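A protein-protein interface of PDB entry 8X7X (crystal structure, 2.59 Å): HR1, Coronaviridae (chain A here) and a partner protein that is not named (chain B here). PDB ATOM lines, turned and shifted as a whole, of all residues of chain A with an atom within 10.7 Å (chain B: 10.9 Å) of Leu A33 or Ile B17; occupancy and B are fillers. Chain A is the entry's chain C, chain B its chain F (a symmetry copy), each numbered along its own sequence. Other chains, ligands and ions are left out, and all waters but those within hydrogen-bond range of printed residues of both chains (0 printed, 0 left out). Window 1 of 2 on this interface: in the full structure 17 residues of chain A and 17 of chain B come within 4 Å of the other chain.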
ATOM      1  N   SER A  23      16.635 -29.853   3.598  1.00  0.00           N
ATOM      2  CA  SER A  23      18.046 -29.951   3.214  1.00  0.00           C
ATOM      3  C   SER A  23      18.233 -29.694   1.721  1.00  0.00           C
ATOM      4  O   SER A  23      18.978 -28.793   1.329  1.00  0.00           O
ATOM      5  CB  SER A  23      18.601 -31.318   3.580  1.00  0.00           C
ATOM      6  OG  SER A  23      20.014 -31.267   3.638  1.00  0.00           O
ATOM      7  N   LEU A  25      16.259 -28.245  -0.325  1.00  0.00           N
ATOM      8  CA  LEU A  25      15.899 -26.859  -0.650  1.00  0.00           C
ATOM      9  C   LEU A  25      17.074 -25.912  -0.412  1.00  0.00           C
ATOM     10  O   LEU A  25      17.421 -25.102  -1.280  1.00  0.00           O
ATOM     11  CB  LEU A  25      14.670 -26.408   0.153  1.00  0.00           C
ATOM     12  CG  LEU A  25      14.295 -24.916   0.070  1.00  0.00           C
ATOM     13  CD1 LEU A  25      14.072 -24.436  -1.391  1.00  0.00           C
ATOM     14  CD2 LEU A  25      13.067 -24.583   0.936  1.00  0.00           C
ATOM     15  N   ALA A  26      17.718 -26.023   0.748  1.00  0.00           N
ATOM     16  CA  ALA A  26      18.849 -25.156   1.055  1.00  0.00           C
ATOM     17  C   ALA A  26      19.992 -25.334   0.052  1.00  0.00           C
ATOM     18  O   ALA A  26      20.553 -24.346  -0.448  1.00  0.00           O
ATOM     19  CB  ALA A  26      19.323 -25.424   2.484  1.00  0.00           C
ATOM     20  N   LEU A  27      20.353 -26.589  -0.253  1.00  0.00           N
ATOM     21  CA  LEU A  27      21.439 -26.833  -1.197  1.00  0.00           C
ATOM     22  C   LEU A  27      21.119 -26.268  -2.581  1.00  0.00           C
ATOM     23  O   LEU A  27      21.968 -25.635  -3.217  1.00  0.00           O
ATOM     24  CB  LEU A  27      21.731 -28.329  -1.273  1.00  0.00           C
ATOM     25  CG  LEU A  27      22.604 -28.802  -0.107  1.00  0.00           C
ATOM     26  CD1 LEU A  27      22.430 -30.269   0.134  1.00  0.00           C
ATOM     27  CD2 LEU A  27      24.050 -28.497  -0.397  1.00  0.00           C
ATOM     28  N   THR A  28      19.892 -26.470  -3.053  1.00  0.00           N
ATOM     29  CA  THR A  28      19.516 -25.958  -4.357  1.00  0.00           C
ATOM     30  C   THR A  28      19.507 -24.436  -4.371  1.00  0.00           C
ATOM     31  O   THR A  28      19.906 -23.820  -5.363  1.00  0.00           O
ATOM     32  CB  THR A  28      18.142 -26.504  -4.739  1.00  0.00           C
ATOM     33  OG1 THR A  28      18.024 -27.862  -4.291  1.00  0.00           O
ATOM     34  CG2 THR A  28      17.932 -26.434  -6.253  1.00  0.00           C
ATOM     35  N   THR A  29      19.064 -23.815  -3.286  1.00  0.00           N
ATOM     36  CA  THR A  29      19.141 -22.366  -3.196  1.00  0.00           C
ATOM     37  C   THR A  29      20.593 -21.895  -3.193  1.00  0.00           C
ATOM     38  O   THR A  29      20.947 -20.935  -3.897  1.00  0.00           O
ATOM     39  CB  THR A  29      18.408 -21.904  -1.941  1.00  0.00           C
ATOM     40  OG1 THR A  29      17.011 -22.113  -2.134  1.00  0.00           O
ATOM     41  CG2 THR A  29      18.658 -20.440  -1.664  1.00  0.00           C
ATOM     42  N   SER A  30      21.443 -22.566  -2.407  1.00  0.00           N
ATOM     43  CA  SER A  30      22.868 -22.268  -2.398  1.00  0.00           C
ATOM     44  C   SER A  30      23.459 -22.331  -3.809  1.00  0.00           C
ATOM     45  O   SER A  30      24.252 -21.465  -4.205  1.00  0.00           O
ATOM     46  CB  SER A  30      23.578 -23.257  -1.472  1.00  0.00           C
ATOM     47  OG  SER A  30      24.983 -23.084  -1.526  1.00  0.00           O
ATOM     48  N   SER A  31      23.073 -23.354  -4.583  1.00  0.00           N
ATOM     49  CA  SER A  31      23.632 -23.555  -5.914  1.00  0.00           C
ATOM     50  C   SER A  31      23.217 -22.437  -6.866  1.00  0.00           C
ATOM     51  O   SER A  31      24.045 -21.930  -7.633  1.00  0.00           O
ATOM     52  CB  SER A  31      23.196 -24.917  -6.448  1.00  0.00           C
ATOM     53  OG  SER A  31      23.622 -25.113  -7.775  1.00  0.00           O
ATOM     54  N   ALA A  32      21.941 -22.037  -6.825  1.00  0.00           N
ATOM     55  CA  ALA A  32      21.480 -20.884  -7.594  1.00  0.00           C
ATOM     56  C   ALA A  32      22.236 -19.617  -7.201  1.00  0.00           C
ATOM     57  O   ALA A  32      22.753 -18.895  -8.069  1.00  0.00           O
ATOM     58  CB  ALA A  32      19.975 -20.694  -7.392  1.00  0.00           C
ATOM     59  N   LEU A  33      22.328 -19.343  -5.891  1.00  0.00           N
ATOM     60  CA  LEU A  33      23.052 -18.162  -5.418  1.00  0.00           C
ATOM     61  C   LEU A  33      24.493 -18.133  -5.931  1.00  0.00           C
ATOM     62  O   LEU A  33      24.984 -17.079  -6.345  1.00  0.00           O
ATOM     63  CB  LEU A  33      23.022 -18.101  -3.888  1.00  0.00           C
ATOM     64  CG  LEU A  33      21.633 -17.838  -3.286  1.00  0.00           C
ATOM     65  CD1 LEU A  33      21.693 -17.764  -1.793  1.00  0.00           C
ATOM     66  CD2 LEU A  33      20.959 -16.565  -3.873  1.00  0.00           C
ATOM     67  N   GLN A  34      25.188 -19.274  -5.916  1.00  0.00           N
ATOM     68  CA  GLN A  34      26.576 -19.295  -6.374  1.00  0.00           C
ATOM     69  C   GLN A  34      26.675 -18.945  -7.847  1.00  0.00           C
ATOM     70  O   GLN A  34      27.553 -18.177  -8.262  1.00  0.00           O
ATOM     71  CB  GLN A  34      27.188 -20.667  -6.123  1.00  0.00           C
ATOM     72  CG  GLN A  34      27.314 -21.022  -4.656  1.00  0.00           C
ATOM     73  CD  GLN A  34      27.728 -22.455  -4.469  1.00  0.00           C
ATOM     74  OE1 GLN A  34      28.613 -22.945  -5.171  1.00  0.00           O
ATOM     75  NE2 GLN A  34      27.088 -23.146  -3.529  1.00  0.00           N
ATOM     76  N   ALA A  35      25.773 -19.496  -8.660  1.00  0.00           N
ATOM     77  CA  ALA A  35      25.812 -19.186 -10.079  1.00  0.00           C
ATOM     78  C   ALA A  35      25.535 -17.708 -10.325  1.00  0.00           C
ATOM     79  O   ALA A  35      26.197 -17.083 -11.155  1.00  0.00           O
ATOM     80  CB  ALA A  35      24.811 -20.058 -10.829  1.00  0.00           C
ATOM     81  N   ILE A  36      24.563 -17.138  -9.604  1.00  0.00           N
ATOM     82  CA  ILE A  36      24.223 -15.723  -9.760  1.00  0.00           C
ATOM     83  C   ILE A  36      25.424 -14.841  -9.426  1.00  0.00           C
ATOM     84  O   ILE A  36      25.747 -13.889 -10.155  1.00  0.00           O
ATOM     85  CB  ILE A  36      23.005 -15.364  -8.890  1.00  0.00           C
ATOM     86  CG1 ILE A  36      21.766 -16.110  -9.408  1.00  0.00           C
ATOM     87  CG2 ILE A  36      22.787 -13.833  -8.897  1.00  0.00           C
ATOM     88  CD1 ILE A  36      20.572 -16.076  -8.488  1.00  0.00           C
ATOM     89  N   GLN A  37      26.107 -15.145  -8.323  1.00  0.00           N
ATOM     90  CA  GLN A  37      27.264 -14.351  -7.950  1.00  0.00           C
ATOM     91  C   GLN A  37      28.323 -14.385  -9.046  1.00  0.00           C
ATOM     92  O   GLN A  37      28.830 -13.342  -9.466  1.00  0.00           O
ATOM     93  CB  GLN A  37      27.839 -14.859  -6.638  1.00  0.00           C
ATOM     94  CG  GLN A  37      28.373 -13.766  -5.763  1.00  0.00           C
ATOM     95  CD  GLN A  37      29.325 -14.269  -4.732  1.00  0.00           C
ATOM     96  OE1 GLN A  37      30.040 -15.252  -4.948  1.00  0.00           O
ATOM     97  NE2 GLN A  37      29.340 -13.608  -3.584  1.00  0.00           N
ATOM     98  N   ALA A  38      28.669 -15.582  -9.518  1.00  0.00           N
ATOM     99  CA  ALA A  38      29.682 -15.706 -10.562  1.00  0.00           C
ATOM    100  C   ALA A  38      29.312 -14.893 -11.805  1.00  0.00           C
ATOM    101  O   ALA A  38      30.132 -14.131 -12.329  1.00  0.00           O
ATOM    102  CB  ALA A  38      29.882 -17.185 -10.911  1.00  0.00           C
ATOM    103  N   VAL A  39      28.065 -15.012 -12.269  1.00  0.00           N
ATOM    104  CA  VAL A  39      27.670 -14.345 -13.506  1.00  0.00           C
ATOM    105  C   VAL A  39      27.604 -12.835 -13.306  1.00  0.00           C
ATOM    106  O   VAL A  39      28.063 -12.062 -14.154  1.00  0.00           O
ATOM    107  CB  VAL A  39      26.331 -14.906 -14.026  1.00  0.00           C
ATOM    108  CG1 VAL A  39      25.777 -14.023 -15.188  1.00  0.00           C
ATOM    109  CG2 VAL A  39      26.485 -16.375 -14.479  1.00  0.00           C
ATOM    110  N   VAL A  40      27.017 -12.386 -12.195  1.00  0.00           N
ATOM    111  CA  VAL A  40      26.856 -10.948 -12.007  1.00  0.00           C
ATOM    112  C   VAL A  40      28.223 -10.276 -11.926  1.00  0.00           C
ATOM    113  O   VAL A  40      28.469  -9.233 -12.564  1.00  0.00           O
ATOM    114  CB  VAL A  40      25.977 -10.653 -10.775  1.00  0.00           C
ATOM    115  CG1 VAL A  40      25.912  -9.137 -10.500  1.00  0.00           C
ATOM    116  CG2 VAL A  40      24.549 -11.205 -10.994  1.00  0.00           C
ATOM    117  N   ASN A  41      29.161 -10.911 -11.216  1.00  0.00           N
ATOM    118  CA  ASN A  41      30.483 -10.323 -11.062  1.00  0.00           C
ATOM    119  C   ASN A  41      31.267 -10.342 -12.376  1.00  0.00           C
ATOM    120  O   ASN A  41      31.956  -9.366 -12.709  1.00  0.00           O
ATOM    121  CB  ASN A  41      31.229 -11.036  -9.932  1.00  0.00           C
ATOM    122  CG  ASN A  41      30.690 -10.649  -8.556  1.00  0.00           C
ATOM    123  OD1 ASN A  41      29.924  -9.682  -8.428  1.00  0.00           O
ATOM    124  ND2 ASN A  41      31.065 -11.407  -7.526  1.00  0.00           N
ATOM    125  N   LEU B  11      29.055  -8.277  -6.358  1.00  0.00           N
ATOM    126  CA  LEU B  11      28.147  -8.966  -5.462  1.00  0.00           C
ATOM    127  C   LEU B  11      28.939  -9.837  -4.501  1.00  0.00           C
ATOM    128  O   LEU B  11      29.789 -10.621  -4.933  1.00  0.00           O
ATOM    129  CB  LEU B  11      27.178  -9.812  -6.278  1.00  0.00           C
ATOM    130  CG  LEU B  11      26.159 -10.644  -5.536  1.00  0.00           C
ATOM    131  CD1 LEU B  11      25.209  -9.736  -4.757  1.00  0.00           C
ATOM    132  CD2 LEU B  11      25.422 -11.496  -6.547  1.00  0.00           C
ATOM    133  N   ASN B  12      28.666  -9.697  -3.199  1.00  0.00           N
ATOM    134  CA  ASN B  12      29.306 -10.513  -2.159  1.00  0.00           C
ATOM    135  C   ASN B  12      28.259 -11.151  -1.252  1.00  0.00           C
ATOM    136  O   ASN B  12      27.793 -10.542  -0.282  1.00  0.00           O
ATOM    137  CB  ASN B  12      30.280  -9.708  -1.338  1.00  0.00           C
ATOM    138  CG  ASN B  12      31.167 -10.592  -0.516  1.00  0.00           C
ATOM    139  OD1 ASN B  12      31.220 -11.798  -0.752  1.00  0.00           O
ATOM    140  ND2 ASN B  12      31.869 -10.019   0.447  1.00  0.00           N
ATOM    141  N   ILE B  13      27.905 -12.391  -1.559  1.00  0.00           N
ATOM    142  CA  ILE B  13      26.967 -13.147  -0.747  1.00  0.00           C
ATOM    143  C   ILE B  13      27.617 -14.482  -0.413  1.00  0.00           C
ATOM    144  O   ILE B  13      26.938 -15.504  -0.277  1.00  0.00           O
ATOM    145  CB  ILE B  13      25.621 -13.303  -1.468  1.00  0.00           C
ATOM    146  CG1 ILE B  13      25.819 -13.969  -2.831  1.00  0.00           C
ATOM    147  CG2 ILE B  13      24.994 -11.925  -1.648  1.00  0.00           C
ATOM    148  CD1 ILE B  13      24.543 -14.206  -3.578  1.00  0.00           C
ATOM    149  N   SER B  14      28.948 -14.475  -0.272  1.00  0.00           N
ATOM    150  CA  SER B  14      29.662 -15.679   0.134  1.00  0.00           C
ATOM    151  C   SER B  14      29.245 -16.135   1.522  1.00  0.00           C
ATOM    152  O   SER B  14      29.153 -17.340   1.774  1.00  0.00           O
ATOM    153  CB  SER B  14      31.172 -15.451   0.087  1.00  0.00           C
ATOM    154  OG  SER B  14      31.629 -15.370  -1.253  1.00  0.00           O
ATOM    155  N   ALA B  15      28.998 -15.193   2.444  1.00  0.00           N
ATOM    156  CA  ALA B  15      28.572 -15.594   3.782  1.00  0.00           C
ATOM    157  C   ALA B  15      27.209 -16.269   3.733  1.00  0.00           C
ATOM    158  O   ALA B  15      27.004 -17.312   4.361  1.00  0.00           O
ATOM    159  CB  ALA B  15      28.532 -14.404   4.742  1.00  0.00           C
ATOM    160  N   GLU B  16      26.264 -15.682   2.992  1.00  0.00           N
ATOM    161  CA  GLU B  16      24.929 -16.269   2.899  1.00  0.00           C
ATOM    162  C   GLU B  16      24.987 -17.656   2.260  1.00  0.00           C
ATOM    163  O   GLU B  16      24.393 -18.612   2.771  1.00  0.00           O
ATOM    164  CB  GLU B  16      23.983 -15.339   2.125  1.00  0.00           C
ATOM    165  CG  GLU B  16      23.577 -14.066   2.894  1.00  0.00           C
ATOM    166  CD  GLU B  16      24.538 -12.907   2.669  1.00  0.00           C
ATOM    167  OE1 GLU B  16      24.133 -11.745   2.903  1.00  0.00           O
ATOM    168  OE2 GLU B  16      25.695 -13.151   2.242  1.00  0.00           O
ATOM    169  N   ILE B  17      25.742 -17.794   1.168  1.00  0.00           N
ATOM    170  CA  ILE B  17      25.942 -19.103   0.548  1.00  0.00           C
ATOM    171  C   ILE B  17      26.474 -20.099   1.572  1.00  0.00           C
ATOM    172  O   ILE B  17      25.958 -21.216   1.723  1.00  0.00           O
ATOM    173  CB  ILE B  17      26.886 -18.962  -0.658  1.00  0.00           C
ATOM    174  CG1 ILE B  17      26.125 -18.296  -1.806  1.00  0.00           C
ATOM    175  CG2 ILE B  17      27.466 -20.308  -1.052  1.00  0.00           C
ATOM    176  CD1 ILE B  17      26.956 -17.889  -2.970  1.00  0.00           C
ATOM    177  N   GLN B  18      27.504 -19.703   2.313  1.00  0.00           N
ATOM    178  CA  GLN B  18      28.117 -20.644   3.236  1.00  0.00           C
ATOM    179  C   GLN B  18      27.223 -20.932   4.433  1.00  0.00           C
ATOM    180  O   GLN B  18      27.224 -22.062   4.945  1.00  0.00           O
ATOM    181  CB  GLN B  18      29.472 -20.124   3.678  1.00  0.00           C
ATOM    182  CG  GLN B  18      29.626 -19.931   5.151  1.00  0.00           C
ATOM    183  CD  GLN B  18      31.032 -20.247   5.592  1.00  0.00           C
ATOM    184  OE1 GLN B  18      31.998 -19.724   5.034  1.00  0.00           O
ATOM    185  NE2 GLN B  18      31.160 -21.131   6.573  1.00  0.00           N
ATOM    186  N   LEU B  19      26.453 -19.939   4.888  1.00  0.00           N
ATOM    187  CA  LEU B  19      25.573 -20.168   6.028  1.00  0.00           C
ATOM    188  C   LEU B  19      24.400 -21.059   5.619  1.00  0.00           C
ATOM    189  O   LEU B  19      23.941 -21.896   6.405  1.00  0.00           O
ATOM    190  CB  LEU B  19      25.106 -18.826   6.615  1.00  0.00           C
ATOM    191  CG  LEU B  19      26.205 -17.978   7.317  1.00  0.00           C
ATOM    192  CD1 LEU B  19      25.893 -16.458   7.421  1.00  0.00           C
ATOM    193  CD2 LEU B  19      26.584 -18.528   8.686  1.00  0.00           C
ATOM    194  N   ILE B  20      23.947 -20.935   4.373  1.00  0.00           N
ATOM    195  CA  ILE B  20      22.908 -21.818   3.863  1.00  0.00           C
ATOM    196  C   ILE B  20      23.436 -23.237   3.683  1.00  0.00           C
ATOM    197  O   ILE B  20      22.697 -24.208   3.876  1.00  0.00           O
ATOM    198  CB  ILE B  20      22.329 -21.236   2.556  1.00  0.00           C
ATOM    199  CG1 ILE B  20      21.486 -19.986   2.877  1.00  0.00           C
ATOM    200  CG2 ILE B  20      21.509 -22.286   1.802  1.00  0.00           C
ATOM    201  CD1 ILE B  20      20.796 -19.345   1.682  1.00  0.00           C
ATOM    202  N   ASN B  21      24.711 -23.397   3.318  1.00  0.00           N
ATOM    203  CA  ASN B  21      25.275 -24.747   3.265  1.00  0.00           C
ATOM    204  C   ASN B  21      25.334 -25.381   4.649  1.00  0.00           C
ATOM    205  O   ASN B  21      25.147 -26.591   4.784  1.00  0.00           O
ATOM    206  CB  ASN B  21      26.673 -24.729   2.636  1.00  0.00           C
ATOM    207  CG  ASN B  21      26.650 -24.399   1.131  1.00  0.00           C
ATOM    208  OD1 ASN B  21      25.609 -24.453   0.479  1.00  0.00           O
ATOM    209  ND2 ASN B  21      27.817 -24.078   0.581  1.00  0.00           N
ATOM    210  N   GLU B  22      25.605 -24.586   5.684  1.00  0.00           N
ATOM    211  CA  GLU B  22      25.649 -25.123   7.034  1.00  0.00           C
ATOM    212  C   GLU B  22      24.259 -25.512   7.517  1.00  0.00           C
ATOM    213  O   GLU B  22      24.105 -26.502   8.250  1.00  0.00           O
ATOM    214  CB  GLU B  22      26.265 -24.103   7.984  1.00  0.00           C
ATOM    215  CG  GLU B  22      27.746 -23.867   7.768  1.00  0.00           C
ATOM    216  CD  GLU B  22      28.309 -22.799   8.701  1.00  0.00           C
ATOM    217  OE1 GLU B  22      27.511 -22.050   9.305  1.00  0.00           O
ATOM    218  OE2 GLU B  22      29.550 -22.709   8.830  1.00  0.00           O
ATOM    219  N   ILE B  23      23.240 -24.748   7.120  1.00  0.00           N
ATOM    220  CA  ILE B  23      21.870 -25.114   7.454  1.00  0.00           C
ATOM    221  C   ILE B  23      21.515 -26.456   6.824  1.00  0.00           C
ATOM    222  O   ILE B  23      20.982 -27.351   7.490  1.00  0.00           O
ATOM    223  CB  ILE B  23      20.904 -23.994   7.030  1.00  0.00           C
ATOM    224  CG1 ILE B  23      21.125 -22.760   7.912  1.00  0.00           C
ATOM    225  CG2 ILE B  23      19.461 -24.450   7.121  1.00  0.00           C
ATOM    226  CD1 ILE B  23      20.197 -21.609   7.597  1.00  0.00           C
ATOM    227  N   ALA B  24      21.831 -26.631   5.534  1.00  0.00           N
ATOM    228  CA  ALA B  24      21.572 -27.905   4.868  1.00  0.00           C
ATOM    229  C   ALA B  24      22.320 -29.067   5.508  1.00  0.00           C
ATOM    230  O   ALA B  24      21.880 -30.216   5.378  1.00  0.00           O
ATOM    231  CB  ALA B  24      21.934 -27.819   3.392  1.00  0.00           C
ATOM    232  N   HIS B  25      23.436 -28.805   6.198  1.00  0.00           N
ATOM    233  CA  HIS B  25      24.133 -29.877   6.905  1.00  0.00           C
ATOM    234  C   HIS B  25      23.543 -30.139   8.294  1.00  0.00           C
ATOM    235  O   HIS B  25      23.510 -31.291   8.738  1.00  0.00           O
ATOM    236  CB  HIS B  25      25.623 -29.549   7.007  1.00  0.00           C
ATOM    237  CG  HIS B  25      26.368 -30.412   7.980  1.00  0.00           C
ATOM    238  ND1 HIS B  25      26.523 -30.072   9.309  1.00  0.00           N
ATOM    239  CD2 HIS B  25      27.002 -31.598   7.822  1.00  0.00           C
ATOM    240  CE1 HIS B  25      27.223 -31.007   9.924  1.00  0.00           C
ATOM    241  NE2 HIS B  25      27.524 -31.946   9.044  1.00  0.00           N
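NE2 of Gln A34 is in hydrogen-bond range of OG of Ser A30 (2.9 Å). The backbone carbonyl oxygen of Ile B17 sits close to the side-chain amide oxygen of Asn B21, at 3.5 Å.
Of the 15 printed residues of chain B, 8 touch a printed residue of chain A. Printed residues of chain B that touch a printed residue of chain A: Leu B11, Asn B12, Ile B13, Ser B14, Ile B17, Ile B20, Asn B21 and Ala B24. Hydrophobic or aromatic side chains of chain B that line the printed part of chain A: Leu B11, Ile B13, Ile B17, Ile B20 and Ala B24. Of the 18 printed residues of chain A, 8 touch a printed residue of chain B. Printed residues of chain A that touch a printed residue of chain B: Ser A23, Ala A26, Leu A27, Ser A30, Leu A33, Gln A34, Gln A37 and Asn A41. Hydrophobic or aromatic side chains of chain A that line the printed part of chain B: Ala A26, Leu A27 and Leu A33.
OG of Ser A23 is in hydrogen-bond range of O of Ala B24 (2.8 Å). NE2 of Gln A37 is in hydrogen-bond range of O of Leu B11, at 3.3 Å. OD1 of Asn A41 is in hydrogen-bond range of N of Leu B11 (2.6 Å). The backbone NH of Ser B14 sits close to the side-chain amide nitrogen of Gln A37 (3.4 Å). The side-chain hydroxyl (OG) of Ser A30 sits at hydrogen-bond distance from the side-chain amide oxygen (OD1) of Asn B21 (2.5 Å). The backbone NH (N) of Ile B13 lies close to the side-chain amide nitrogen (NE2) of Gln A37 (2.8 Å).
Printed residues of chain B within 4 Å of Leu A33: Ile B17 (3.7 Å) and Ile B20 (3.9 Å). Of chain A, only Ser A30, Leu A33 and Gln A34 come within 4 Å of Ile B17. No residue of chain B comes within 4 Å of Thr A29. No residue of chain B comes within 4 Å of Ala A32. No residue of chain B comes within 4 Å of Ala A35. Of chain B, only Leu B11 (3.3 Å), Asn B12 (3.4 Å), Ile B13 (2.8 Å) and Ser B14 (3.4 Å) come within 4 Å of Gln A37. Ser B14 touches one residue of chain A. Ala B15 touches none of the printed residues of chain A. No residue of chain A comes within 4 Å of Glu B16. Of the printed residues of chain B, Leu A27 touches Ala B24 (3.7 Å). Of the printed residues of chain A, Ile B13 touches Gln A37 (2.8 Å). Thr A28 touches none of the printed residues of chain B. Leu B19 touches none of the printed residues of chain A. The nearest printed residue of chain B that does not touch Leu A27 is Asn B21 (4.4 Å).
Among the printed residues, pairs that only touch across the chains: Ala A26 with Ile B20 (3.2 Å), Gln A37 with Asn B12 (3.4 Å), Gln A34 with Ile B17 (3.6 Å), Ala A26 with Ala B24 (3.7 Å), Leu A27 with Ala B24 (3.7 Å), Leu A33 with Ile B17 (3.7 Å), Ser A30 with Ile B17 (3.8 Å), Leu A33 with Ile B20 (3.9 Å) and Ser A30 with Ile B20 (3.99 Å).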
